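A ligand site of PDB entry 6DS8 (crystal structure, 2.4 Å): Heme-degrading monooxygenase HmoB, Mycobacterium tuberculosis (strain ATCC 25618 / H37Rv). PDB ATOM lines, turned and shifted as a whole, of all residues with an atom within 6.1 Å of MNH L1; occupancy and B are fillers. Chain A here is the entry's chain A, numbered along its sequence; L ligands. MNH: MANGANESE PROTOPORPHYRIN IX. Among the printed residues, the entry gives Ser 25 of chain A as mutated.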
ATOM      1  N   ARG A  21      -7.046  17.355  13.532  1.00  0.00           N
ATOM      2  CA  ARG A  21      -6.144  18.467  13.787  1.00  0.00           C
ATOM      3  C   ARG A  21      -6.845  19.591  14.544  1.00  0.00           C
ATOM      4  O   ARG A  21      -6.208  20.311  15.307  1.00  0.00           O
ATOM      5  CB  ARG A  21      -5.523  18.937  12.472  1.00  0.00           C
ATOM      6  CG  ARG A  21      -4.695  17.848  11.838  1.00  0.00           C
ATOM      7  CD  ARG A  21      -3.970  18.297  10.624  1.00  0.00           C
ATOM      8  NE  ARG A  21      -3.076  17.254  10.148  1.00  0.00           N
ATOM      9  CZ  ARG A  21      -2.220  17.402   9.133  1.00  0.00           C
ATOM     10  NH1 ARG A  21      -2.131  18.555   8.484  1.00  0.00           N
ATOM     11  NH2 ARG A  21      -1.453  16.381   8.749  1.00  0.00           N
ATOM     12  N   HIS A  24      -8.245  19.369  19.300  1.00  0.00           N
ATOM     13  CA  HIS A  24      -7.682  19.821  20.559  1.00  0.00           C
ATOM     14  C   HIS A  24      -7.044  21.209  20.452  1.00  0.00           C
ATOM     15  O   HIS A  24      -6.046  21.526  21.112  1.00  0.00           O
ATOM     16  CB  HIS A  24      -6.714  18.762  21.096  1.00  0.00           C
ATOM     17  CG  HIS A  24      -7.418  17.478  21.445  1.00  0.00           C
ATOM     18  ND1 HIS A  24      -7.119  16.267  20.869  1.00  0.00           N
ATOM     19  CD2 HIS A  24      -8.461  17.239  22.282  1.00  0.00           C
ATOM     20  CE1 HIS A  24      -7.919  15.334  21.350  1.00  0.00           C
ATOM     21  NE2 HIS A  24      -8.748  15.904  22.213  1.00  0.00           N
ATOM     22  N   SER A  25      -7.665  22.068  19.643  1.00  0.00           N
ATOM     23  CA  SER A  25      -7.112  23.370  19.352  1.00  0.00           C
ATOM     24  C   SER A  25      -7.753  24.485  20.171  1.00  0.00           C
ATOM     25  O   SER A  25      -7.334  25.645  20.037  1.00  0.00           O
ATOM     26  CB  SER A  25      -7.270  23.661  17.852  1.00  0.00           C
ATOM     27  OG  SER A  25      -8.628  23.797  17.465  1.00  0.00           O
ATOM     28  N   ALA A  26      -8.738  24.152  21.027  1.00  0.00           N
ATOM     29  CA  ALA A  26      -9.464  25.176  21.777  1.00  0.00           C
ATOM     30  C   ALA A  26      -8.535  26.140  22.512  1.00  0.00           C
ATOM     31  O   ALA A  26      -8.777  27.356  22.534  1.00  0.00           O
ATOM     32  CB  ALA A  26     -10.403  24.506  22.784  1.00  0.00           C
ATOM     33  N   HIS A  27      -7.460  25.620  23.120  1.00  0.00           N
ATOM     34  CA  HIS A  27      -6.575  26.407  23.957  1.00  0.00           C
ATOM     35  C   HIS A  27      -5.958  27.594  23.216  1.00  0.00           C
ATOM     36  O   HIS A  27      -5.604  28.596  23.834  1.00  0.00           O
ATOM     37  CB  HIS A  27      -5.470  25.509  24.528  1.00  0.00           C
ATOM     38  CG  HIS A  27      -4.527  24.981  23.480  1.00  0.00           C
ATOM     39  ND1 HIS A  27      -3.226  25.448  23.347  1.00  0.00           N
ATOM     40  CD2 HIS A  27      -4.702  24.060  22.512  1.00  0.00           C
ATOM     41  CE1 HIS A  27      -2.646  24.822  22.339  1.00  0.00           C
ATOM     42  NE2 HIS A  27      -3.511  23.972  21.810  1.00  0.00           N
ATOM     43  N   ALA A  28      -5.808  27.482  21.892  1.00  0.00           N
ATOM     44  CA  ALA A  28      -5.089  28.449  21.080  1.00  0.00           C
ATOM     45  C   ALA A  28      -5.858  29.752  20.865  1.00  0.00           C
ATOM     46  O   ALA A  28      -5.299  30.704  20.322  1.00  0.00           O
ATOM     47  CB  ALA A  28      -4.756  27.810  19.718  1.00  0.00           C
ATOM     48  N   VAL A  29      -7.141  29.785  21.190  1.00  0.00           N
ATOM     49  CA  VAL A  29      -7.959  30.947  20.866  1.00  0.00           C
ATOM     50  C   VAL A  29      -8.938  31.249  21.998  1.00  0.00           C
ATOM     51  O   VAL A  29      -9.528  32.333  22.078  1.00  0.00           O
ATOM     52  CB  VAL A  29      -8.671  30.722  19.510  1.00  0.00           C
ATOM     53  CG1 VAL A  29      -9.774  29.650  19.673  1.00  0.00           C
ATOM     54  CG2 VAL A  29      -9.192  32.036  18.952  1.00  0.00           C
ATOM     55  N   PHE A  62      -9.885  40.404  16.263  1.00  0.00           N
ATOM     56  CA  PHE A  62      -9.484  39.305  15.391  1.00  0.00           C
ATOM     57  C   PHE A  62      -8.051  39.489  14.906  1.00  0.00           C
ATOM     58  O   PHE A  62      -7.250  38.543  14.948  1.00  0.00           O
ATOM     59  CB  PHE A  62     -10.428  39.157  14.197  1.00  0.00           C
ATOM     60  CG  PHE A  62      -9.850  38.349  13.076  1.00  0.00           C
ATOM     61  CD1 PHE A  62      -9.726  36.967  13.203  1.00  0.00           C
ATOM     62  CD2 PHE A  62      -9.341  38.973  11.924  1.00  0.00           C
ATOM     63  CE1 PHE A  62      -9.139  36.227  12.183  1.00  0.00           C
ATOM     64  CE2 PHE A  62      -8.762  38.229  10.903  1.00  0.00           C
ATOM     65  CZ  PHE A  62      -8.666  36.846  11.049  1.00  0.00           C
ATOM     66  N   TRP A  65      -5.359  38.609  17.557  1.00  0.00           N
ATOM     67  CA  TRP A  65      -5.126  37.182  17.722  1.00  0.00           C
ATOM     68  C   TRP A  65      -4.371  36.611  16.535  1.00  0.00           C
ATOM     69  O   TRP A  65      -3.405  35.858  16.709  1.00  0.00           O
ATOM     70  CB  TRP A  65      -6.459  36.448  17.923  1.00  0.00           C
ATOM     71  CG  TRP A  65      -6.303  34.984  17.954  1.00  0.00           C
ATOM     72  CD1 TRP A  65      -5.794  34.236  18.976  1.00  0.00           C
ATOM     73  CD2 TRP A  65      -6.640  34.049  16.913  1.00  0.00           C
ATOM     74  NE1 TRP A  65      -5.785  32.903  18.636  1.00  0.00           N
ATOM     75  CE2 TRP A  65      -6.318  32.755  17.378  1.00  0.00           C
ATOM     76  CE3 TRP A  65      -7.193  34.185  15.624  1.00  0.00           C
ATOM     77  CZ2 TRP A  65      -6.507  31.603  16.610  1.00  0.00           C
ATOM     78  CZ3 TRP A  65      -7.410  33.040  14.858  1.00  0.00           C
ATOM     79  CH2 TRP A  65      -7.058  31.765  15.352  1.00  0.00           C
ATOM     80  N   ALA A  66      -4.781  36.985  15.319  1.00  0.00           N
ATOM     81  CA  ALA A  66      -4.191  36.430  14.103  1.00  0.00           C
ATOM     82  C   ALA A  66      -2.704  36.754  14.005  1.00  0.00           C
ATOM     83  O   ALA A  66      -1.921  35.917  13.520  1.00  0.00           O
ATOM     84  CB  ALA A  66      -4.930  36.981  12.882  1.00  0.00           C
ATOM     85  N   ASN A  67      -2.283  37.921  14.494  1.00  0.00           N
ATOM     86  CA  ASN A  67      -0.897  38.325  14.339  1.00  0.00           C
ATOM     87  C   ASN A  67       0.030  37.861  15.447  1.00  0.00           C
ATOM     88  O   ASN A  67       1.247  37.794  15.236  1.00  0.00           O
ATOM     89  CB  ASN A  67      -0.836  39.837  14.214  1.00  0.00           C
ATOM     90  CG  ASN A  67      -1.687  40.321  13.083  1.00  0.00           C
ATOM     91  OD1 ASN A  67      -1.816  39.633  12.066  1.00  0.00           O
ATOM     92  ND2 ASN A  67      -2.301  41.498  13.241  1.00  0.00           N
ATOM     93  N   ALA A  70      -1.915  33.329  17.520  1.00  0.00           N
ATOM     94  CA  ALA A  70      -2.191  32.345  16.482  1.00  0.00           C
ATOM     95  C   ALA A  70      -0.896  31.817  15.871  1.00  0.00           C
ATOM     96  O   ALA A  70      -0.732  30.593  15.706  1.00  0.00           O
ATOM     97  CB  ALA A  70      -3.111  32.947  15.417  1.00  0.00           C
ATOM     98  N   ALA A  73       0.952  29.724  18.508  1.00  0.00           N
ATOM     99  CA  ALA A  73       0.368  28.416  18.796  1.00  0.00           C
ATOM    100  C   ALA A  73       0.857  27.310  17.859  1.00  0.00           C
ATOM    101  O   ALA A  73       0.468  26.149  18.015  1.00  0.00           O
ATOM    102  CB  ALA A  73      -1.172  28.486  18.744  1.00  0.00           C
ATOM    103  N   HIS A  74       1.710  27.671  16.903  1.00  0.00           N
ATOM    104  CA  HIS A  74       2.315  26.743  15.951  1.00  0.00           C
ATOM    105  C   HIS A  74       3.628  26.156  16.442  1.00  0.00           C
ATOM    106  O   HIS A  74       4.210  25.339  15.725  1.00  0.00           O
ATOM    107  CB  HIS A  74       2.607  27.452  14.633  1.00  0.00           C
ATOM    108  CG  HIS A  74       1.400  27.739  13.794  1.00  0.00           C
ATOM    109  ND1 HIS A  74       0.796  28.979  13.762  1.00  0.00           N
ATOM    110  CD2 HIS A  74       0.713  26.965  12.923  1.00  0.00           C
ATOM    111  CE1 HIS A  74      -0.221  28.941  12.920  1.00  0.00           C
ATOM    112  NE2 HIS A  74      -0.283  27.732  12.391  1.00  0.00           N
ATOM    113  N   HIS A  77       4.213  22.331  16.350  1.00  0.00           N
ATOM    114  CA  HIS A  77       3.692  21.571  15.189  1.00  0.00           C
ATOM    115  C   HIS A  77       4.446  21.692  13.871  1.00  0.00           C
ATOM    116  O   HIS A  77       5.164  22.664  13.650  1.00  0.00           O
ATOM    117  CB  HIS A  77       2.264  22.020  14.909  1.00  0.00           C
ATOM    118  CG  HIS A  77       1.411  22.063  16.116  1.00  0.00           C
ATOM    119  ND1 HIS A  77       0.456  21.131  16.358  1.00  0.00           N
ATOM    120  CD2 HIS A  77       1.377  22.910  17.158  1.00  0.00           C
ATOM    121  CE1 HIS A  77      -0.148  21.406  17.499  1.00  0.00           C
ATOM    122  NE2 HIS A  77       0.412  22.483  18.000  1.00  0.00           N
ATOM    123  N   ARG A  78       4.179  20.726  13.001  1.00  0.00           N
ATOM    124  CA  ARG A  78       4.659  20.707  11.592  1.00  0.00           C
ATOM    125  C   ARG A  78       3.811  21.721  10.846  1.00  0.00           C
ATOM    126  O   ARG A  78       2.660  21.924  11.207  1.00  0.00           O
ATOM    127  CB  ARG A  78       4.279  19.408  10.891  1.00  0.00           C
ATOM    128  CG  ARG A  78       5.040  18.158  11.319  1.00  0.00           C
ATOM    129  CD  ARG A  78       4.326  17.447  12.454  1.00  0.00           C
ATOM    130  NE  ARG A  78       3.249  18.206  13.084  1.00  0.00           N
ATOM    131  CZ  ARG A  78       3.077  18.323  14.389  1.00  0.00           C
ATOM    132  NH1 ARG A  78       4.038  17.956  15.225  1.00  0.00           N
ATOM    133  NH2 ARG A  78       1.945  18.783  14.860  1.00  0.00           N
ATOM    134  N   ALA A  79       4.316  22.253   9.734  1.00  0.00           N
ATOM    135  CA  ALA A  79       3.498  23.218   8.971  1.00  0.00           C
ATOM    136  C   ALA A  79       2.943  22.561   7.709  1.00  0.00           C
ATOM    137  O   ALA A  79       2.527  23.287   6.842  1.00  0.00           O
ATOM    138  CB  ALA A  79       4.311  24.454   8.671  1.00  0.00           C
ATOM    139  N   ASN A  80       2.943  21.224   7.667  1.00  0.00           N
ATOM    140  CA  ASN A  80       2.485  20.423   6.525  1.00  0.00           C
ATOM    141  C   ASN A  80       0.960  20.276   6.518  1.00  0.00           C
ATOM    142  O   ASN A  80       0.409  19.424   7.239  1.00  0.00           O
ATOM    143  CB  ASN A  80       3.148  19.042   6.535  1.00  0.00           C
ATOM    144  CG  ASN A  80       2.999  18.277   5.188  1.00  0.00           C
ATOM    145  OD1 ASN A  80       2.378  18.755   4.233  1.00  0.00           O
ATOM    146  ND2 ASN A  80       3.569  17.070   5.136  1.00  0.00           N
ATOM    147  N   PRO A  81       0.221  21.034   5.709  1.00  0.00           N
ATOM    148  CA  PRO A  81      -1.225  20.963   5.733  1.00  0.00           C
ATOM    149  C   PRO A  81      -1.936  19.818   4.988  1.00  0.00           C
ATOM    150  O   PRO A  81      -1.396  19.227   4.121  1.00  0.00           O
ATOM    151  CB  PRO A  81      -1.581  22.297   5.069  1.00  0.00           C
ATOM    152  CG  PRO A  81      -0.518  22.483   4.073  1.00  0.00           C
ATOM    153  CD  PRO A  81       0.723  21.993   4.749  1.00  0.00           C
ATOM    154  N   VAL A  82      -3.127  19.496   5.458  1.00  0.00           N
ATOM    155  CA  VAL A  82      -3.975  18.532   4.725  1.00  0.00           C
ATOM    156  C   VAL A  82      -4.829  19.366   3.782  1.00  0.00           C
ATOM    157  O   VAL A  82      -5.118  18.911   2.701  1.00  0.00           O
ATOM    158  CB  VAL A  82      -4.774  17.617   5.662  1.00  0.00           C
ATOM    159  CG1 VAL A  82      -5.681  18.354   6.609  1.00  0.00           C
ATOM    160  CG2 VAL A  82      -5.558  16.569   4.899  1.00  0.00           C
HETATM  161 MN   MNH L   1      -2.285  27.159  10.999  1.00  0.00          MN
HETATM  162  CHA MNH L   1      -2.549  24.720  12.917  1.00  0.00           C
HETATM  163  CHB MNH L   1      -0.635  25.491   8.909  1.00  0.00           C
HETATM  164  CHC MNH L   1      -1.892  29.789   9.017  1.00  0.00           C
HETATM  165  CHD MNH L   1      -4.001  28.896  12.856  1.00  0.00           C
HETATM  166  NA  MNH L   1      -1.287  25.367  11.085  1.00  0.00           N
HETATM  167  C1A MNH L   1      -1.735  24.327  11.854  1.00  0.00           C
HETATM  168  C2A MNH L   1      -1.301  23.089  11.314  1.00  0.00           C
HETATM  169  C3A MNH L   1      -0.773  23.291  10.129  1.00  0.00           C
HETATM  170  C4A MNH L   1      -0.862  24.699   9.992  1.00  0.00           C
HETATM  171  CMA MNH L   1      -0.205  22.353   9.108  1.00  0.00           C
HETATM  172  CAA MNH L   1      -1.559  21.755  11.964  1.00  0.00           C
HETATM  173  CBA MNH L   1      -0.660  21.431  13.114  1.00  0.00           C
HETATM  174  CGA MNH L   1      -0.844  20.154  13.906  1.00  0.00           C
HETATM  175  O1A MNH L   1      -1.668  20.100  14.819  1.00  0.00           O
HETATM  176  O2A MNH L   1      -0.098  19.248  13.544  1.00  0.00           O
HETATM  177  NB  MNH L   1      -1.145  27.656   9.191  1.00  0.00           N
HETATM  178  C1B MNH L   1      -0.593  26.749   8.364  1.00  0.00           C
HETATM  179  C2B MNH L   1       0.003  27.221   7.199  1.00  0.00           C
HETATM  180  C3B MNH L   1      -0.352  28.503   7.350  1.00  0.00           C
HETATM  181  C4B MNH L   1      -1.115  28.790   8.491  1.00  0.00           C
HETATM  182  CMB MNH L   1       0.747  26.308   6.212  1.00  0.00           C
HETATM  183  CAB MNH L   1      -0.004  29.532   6.338  1.00  0.00           C
HETATM  184  CBB MNH L   1       0.976  29.932   5.294  1.00  0.00           C
HETATM  185  NC  MNH L   1      -2.941  29.192  10.917  1.00  0.00           N
HETATM  186  C1C MNH L   1      -2.733  30.153  10.015  1.00  0.00           C
HETATM  187  C2C MNH L   1      -3.520  31.305  10.278  1.00  0.00           C
HETATM  188  C3C MNH L   1      -4.162  31.047  11.385  1.00  0.00           C
HETATM  189  C4C MNH L   1      -3.796  29.740  11.792  1.00  0.00           C
HETATM  190  CMC MNH L   1      -3.486  32.558   9.431  1.00  0.00           C
HETATM  191  CAC MNH L   1      -5.099  31.934  12.110  1.00  0.00           C
HETATM  192  CBC MNH L   1      -5.125  33.393  12.283  1.00  0.00           C
HETATM  193  ND  MNH L   1      -3.030  26.936  12.910  1.00  0.00           N
HETATM  194  C1D MNH L   1      -3.775  27.780  13.612  1.00  0.00           C
HETATM  195  C2D MNH L   1      -4.223  27.263  14.849  1.00  0.00           C
HETATM  196  C3D MNH L   1      -3.838  25.985  14.807  1.00  0.00           C
HETATM  197  C4D MNH L   1      -3.157  25.775  13.586  1.00  0.00           C
HETATM  198  CMD MNH L   1      -4.959  28.038  15.922  1.00  0.00           C
HETATM  199  CAD MNH L   1      -4.082  24.967  15.900  1.00  0.00           C
HETATM  200  CBD MNH L   1      -2.997  24.960  16.952  1.00  0.00           C
HETATM  201  CGD MNH L   1      -2.947  23.878  17.984  1.00  0.00           C
HETATM  202  O1D MNH L   1      -3.652  22.889  18.038  1.00  0.00           O
HETATM  203  O2D MNH L   1      -2.114  24.026  18.853  1.00  0.00           O
HETATM  204 MN   MNH L   2      -6.749  28.156  10.461  1.00  0.00          MN
HETATM  205  CHA MNH L   2      -4.673  26.224   8.912  1.00  0.00           C
HETATM  206  CHB MNH L   2      -5.976  30.598   8.299  1.00  0.00           C
HETATM  207  CHC MNH L   2      -8.650  30.346  12.049  1.00  0.00           C
HETATM  208  CHD MNH L   2      -6.784  26.254  12.934  1.00  0.00           C
HETATM  209  NA  MNH L   2      -5.406  28.410   8.855  1.00  0.00           N
HETATM  210  C1A MNH L   2      -4.751  27.399   8.183  1.00  0.00           C
HETATM  211  C2A MNH L   2      -4.222  27.870   6.908  1.00  0.00           C
HETATM  212  C3A MNH L   2      -4.449  29.188   6.776  1.00  0.00           C
HETATM  213  C4A MNH L   2      -5.254  29.470   7.958  1.00  0.00           C
HETATM  214  CMA MNH L   2      -4.112  30.173   5.662  1.00  0.00           C
HETATM  215  CAA MNH L   2      -3.430  26.919   6.005  1.00  0.00           C
HETATM  216  CBA MNH L   2      -4.344  26.253   4.957  1.00  0.00           C
HETATM  217  CGA MNH L   2      -3.712  25.617   3.699  1.00  0.00           C
HETATM  218  O1A MNH L   2      -2.537  25.198   3.695  1.00  0.00           O
HETATM  219  O2A MNH L   2      -4.488  25.588   2.706  1.00  0.00           O
HETATM  220  NB  MNH L   2      -7.229  30.278  10.171  1.00  0.00           N
HETATM  221  C1B MNH L   2      -6.835  31.184   9.200  1.00  0.00           C
HETATM  222  C2B MNH L   2      -7.541  32.453   9.187  1.00  0.00           C
HETATM  223  C3B MNH L   2      -8.471  32.151  10.185  1.00  0.00           C
HETATM  224  C4B MNH L   2      -8.217  30.927  10.879  1.00  0.00           C
HETATM  225  CMB MNH L   2      -7.272  33.505   8.108  1.00  0.00           C
HETATM  226  CAB MNH L   2      -9.603  33.008  10.723  1.00  0.00           C
HETATM  227  CBB MNH L   2     -11.103  32.874  10.925  1.00  0.00           C
HETATM  228  NC  MNH L   2      -7.532  28.357  12.437  1.00  0.00           N
HETATM  229  C1C MNH L   2      -8.466  29.270  12.894  1.00  0.00           C
HETATM  230  C2C MNH L   2      -8.933  28.920  14.216  1.00  0.00           C
HETATM  231  C3C MNH L   2      -8.380  27.731  14.491  1.00  0.00           C
HETATM  232  C4C MNH L   2      -7.523  27.349  13.369  1.00  0.00           C
HETATM  233  CMC MNH L   2     -10.023  29.710  14.976  1.00  0.00           C
HETATM  234  CAC MNH L   2      -8.631  26.863  15.706  1.00  0.00           C
HETATM  235  CBC MNH L   2      -8.005  27.034  17.061  1.00  0.00           C
HETATM  236  ND  MNH L   2      -5.821  26.353  10.927  1.00  0.00           N
HETATM  237  C1D MNH L   2      -6.077  25.530  12.009  1.00  0.00           C
HETATM  238  C2D MNH L   2      -5.486  24.197  11.865  1.00  0.00           C
HETATM  239  C3D MNH L   2      -4.791  24.295  10.709  1.00  0.00           C
HETATM  240  C4D MNH L   2      -5.030  25.582  10.104  1.00  0.00           C
HETATM  241  CMD MNH L   2      -5.608  23.036  12.820  1.00  0.00           C
HETATM  242  CAD MNH L   2      -4.107  23.158   9.957  1.00  0.00           C
HETATM  243  CBD MNH L   2      -5.033  22.644   8.848  1.00  0.00           C
HETATM  244  CGD MNH L   2      -4.513  21.530   7.951  1.00  0.00           C
HETATM  245  O1D MNH L   2      -3.700  20.687   8.343  1.00  0.00           O
HETATM  246  O2D MNH L   2      -4.948  21.494   6.760  1.00  0.00           O
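The guanidinium group of Arg 78 is in salt-bridge range of an oxygen (O2A) of MNH L1.
A ring nitrogen (NE2) of His 74 is bound to a manganese atom (MN) of MNH L1, 2.5 Å away.
A ring nitrogen (ND1) of His 77 sits at hydrogen-bond distance from an oxygen (O1A) of MNH L1 (2.8 Å).
A ring nitrogen (NE2) of His 27 sits at hydrogen-bond distance from an oxygen (O2D) of MNH L1 (3.3 Å).
O1D of MNH L2 is in salt-bridge range of NH1 of Arg 21 (2.7 Å).
An oxygen (O2D) of MNH L2 is in hydrogen-bond range of the backbone NH of Val 82, 3.0 Å away.
O of Ala 73 lies close to O2D of MNH L1 (3.4 Å).
Residues that only touch MNH L1: Ala 79, Trp 65, Asn 80, Ala 66, Pro 81, Ser 25, Ala 70 and Ala 28.
Hydrophobic or aromatic side chains within 4 Å of MNH L1: His 27, Ala 28, Trp 65, Ala 66, Ala 70, His 74 and His 77.
Within 4 Å of MNH L1: Ser 25, His 27, Ala 28, Trp 65, Ala 66, Ala 70, Ala 73, His 74, His 77, Arg 78, Ala 79, Asn 80 and Pro 81.
NH2 of Arg 78 lies within hydrogen-bond range of ND1 of His 77.
O of Ala 70 sits at hydrogen-bond distance from ND1 of His 74 (3.0 Å).
The backbone NH of Ala 70 lies within hydrogen-bond range of the backbone carbonyl oxygen of Trp 65.
NE1 of Trp 65 sits at hydrogen-bond distance from O of Ala 28 (2.8 Å).
O of Asn 80 sits at hydrogen-bond distance from NH1 of Arg 21, 3.0 Å away.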
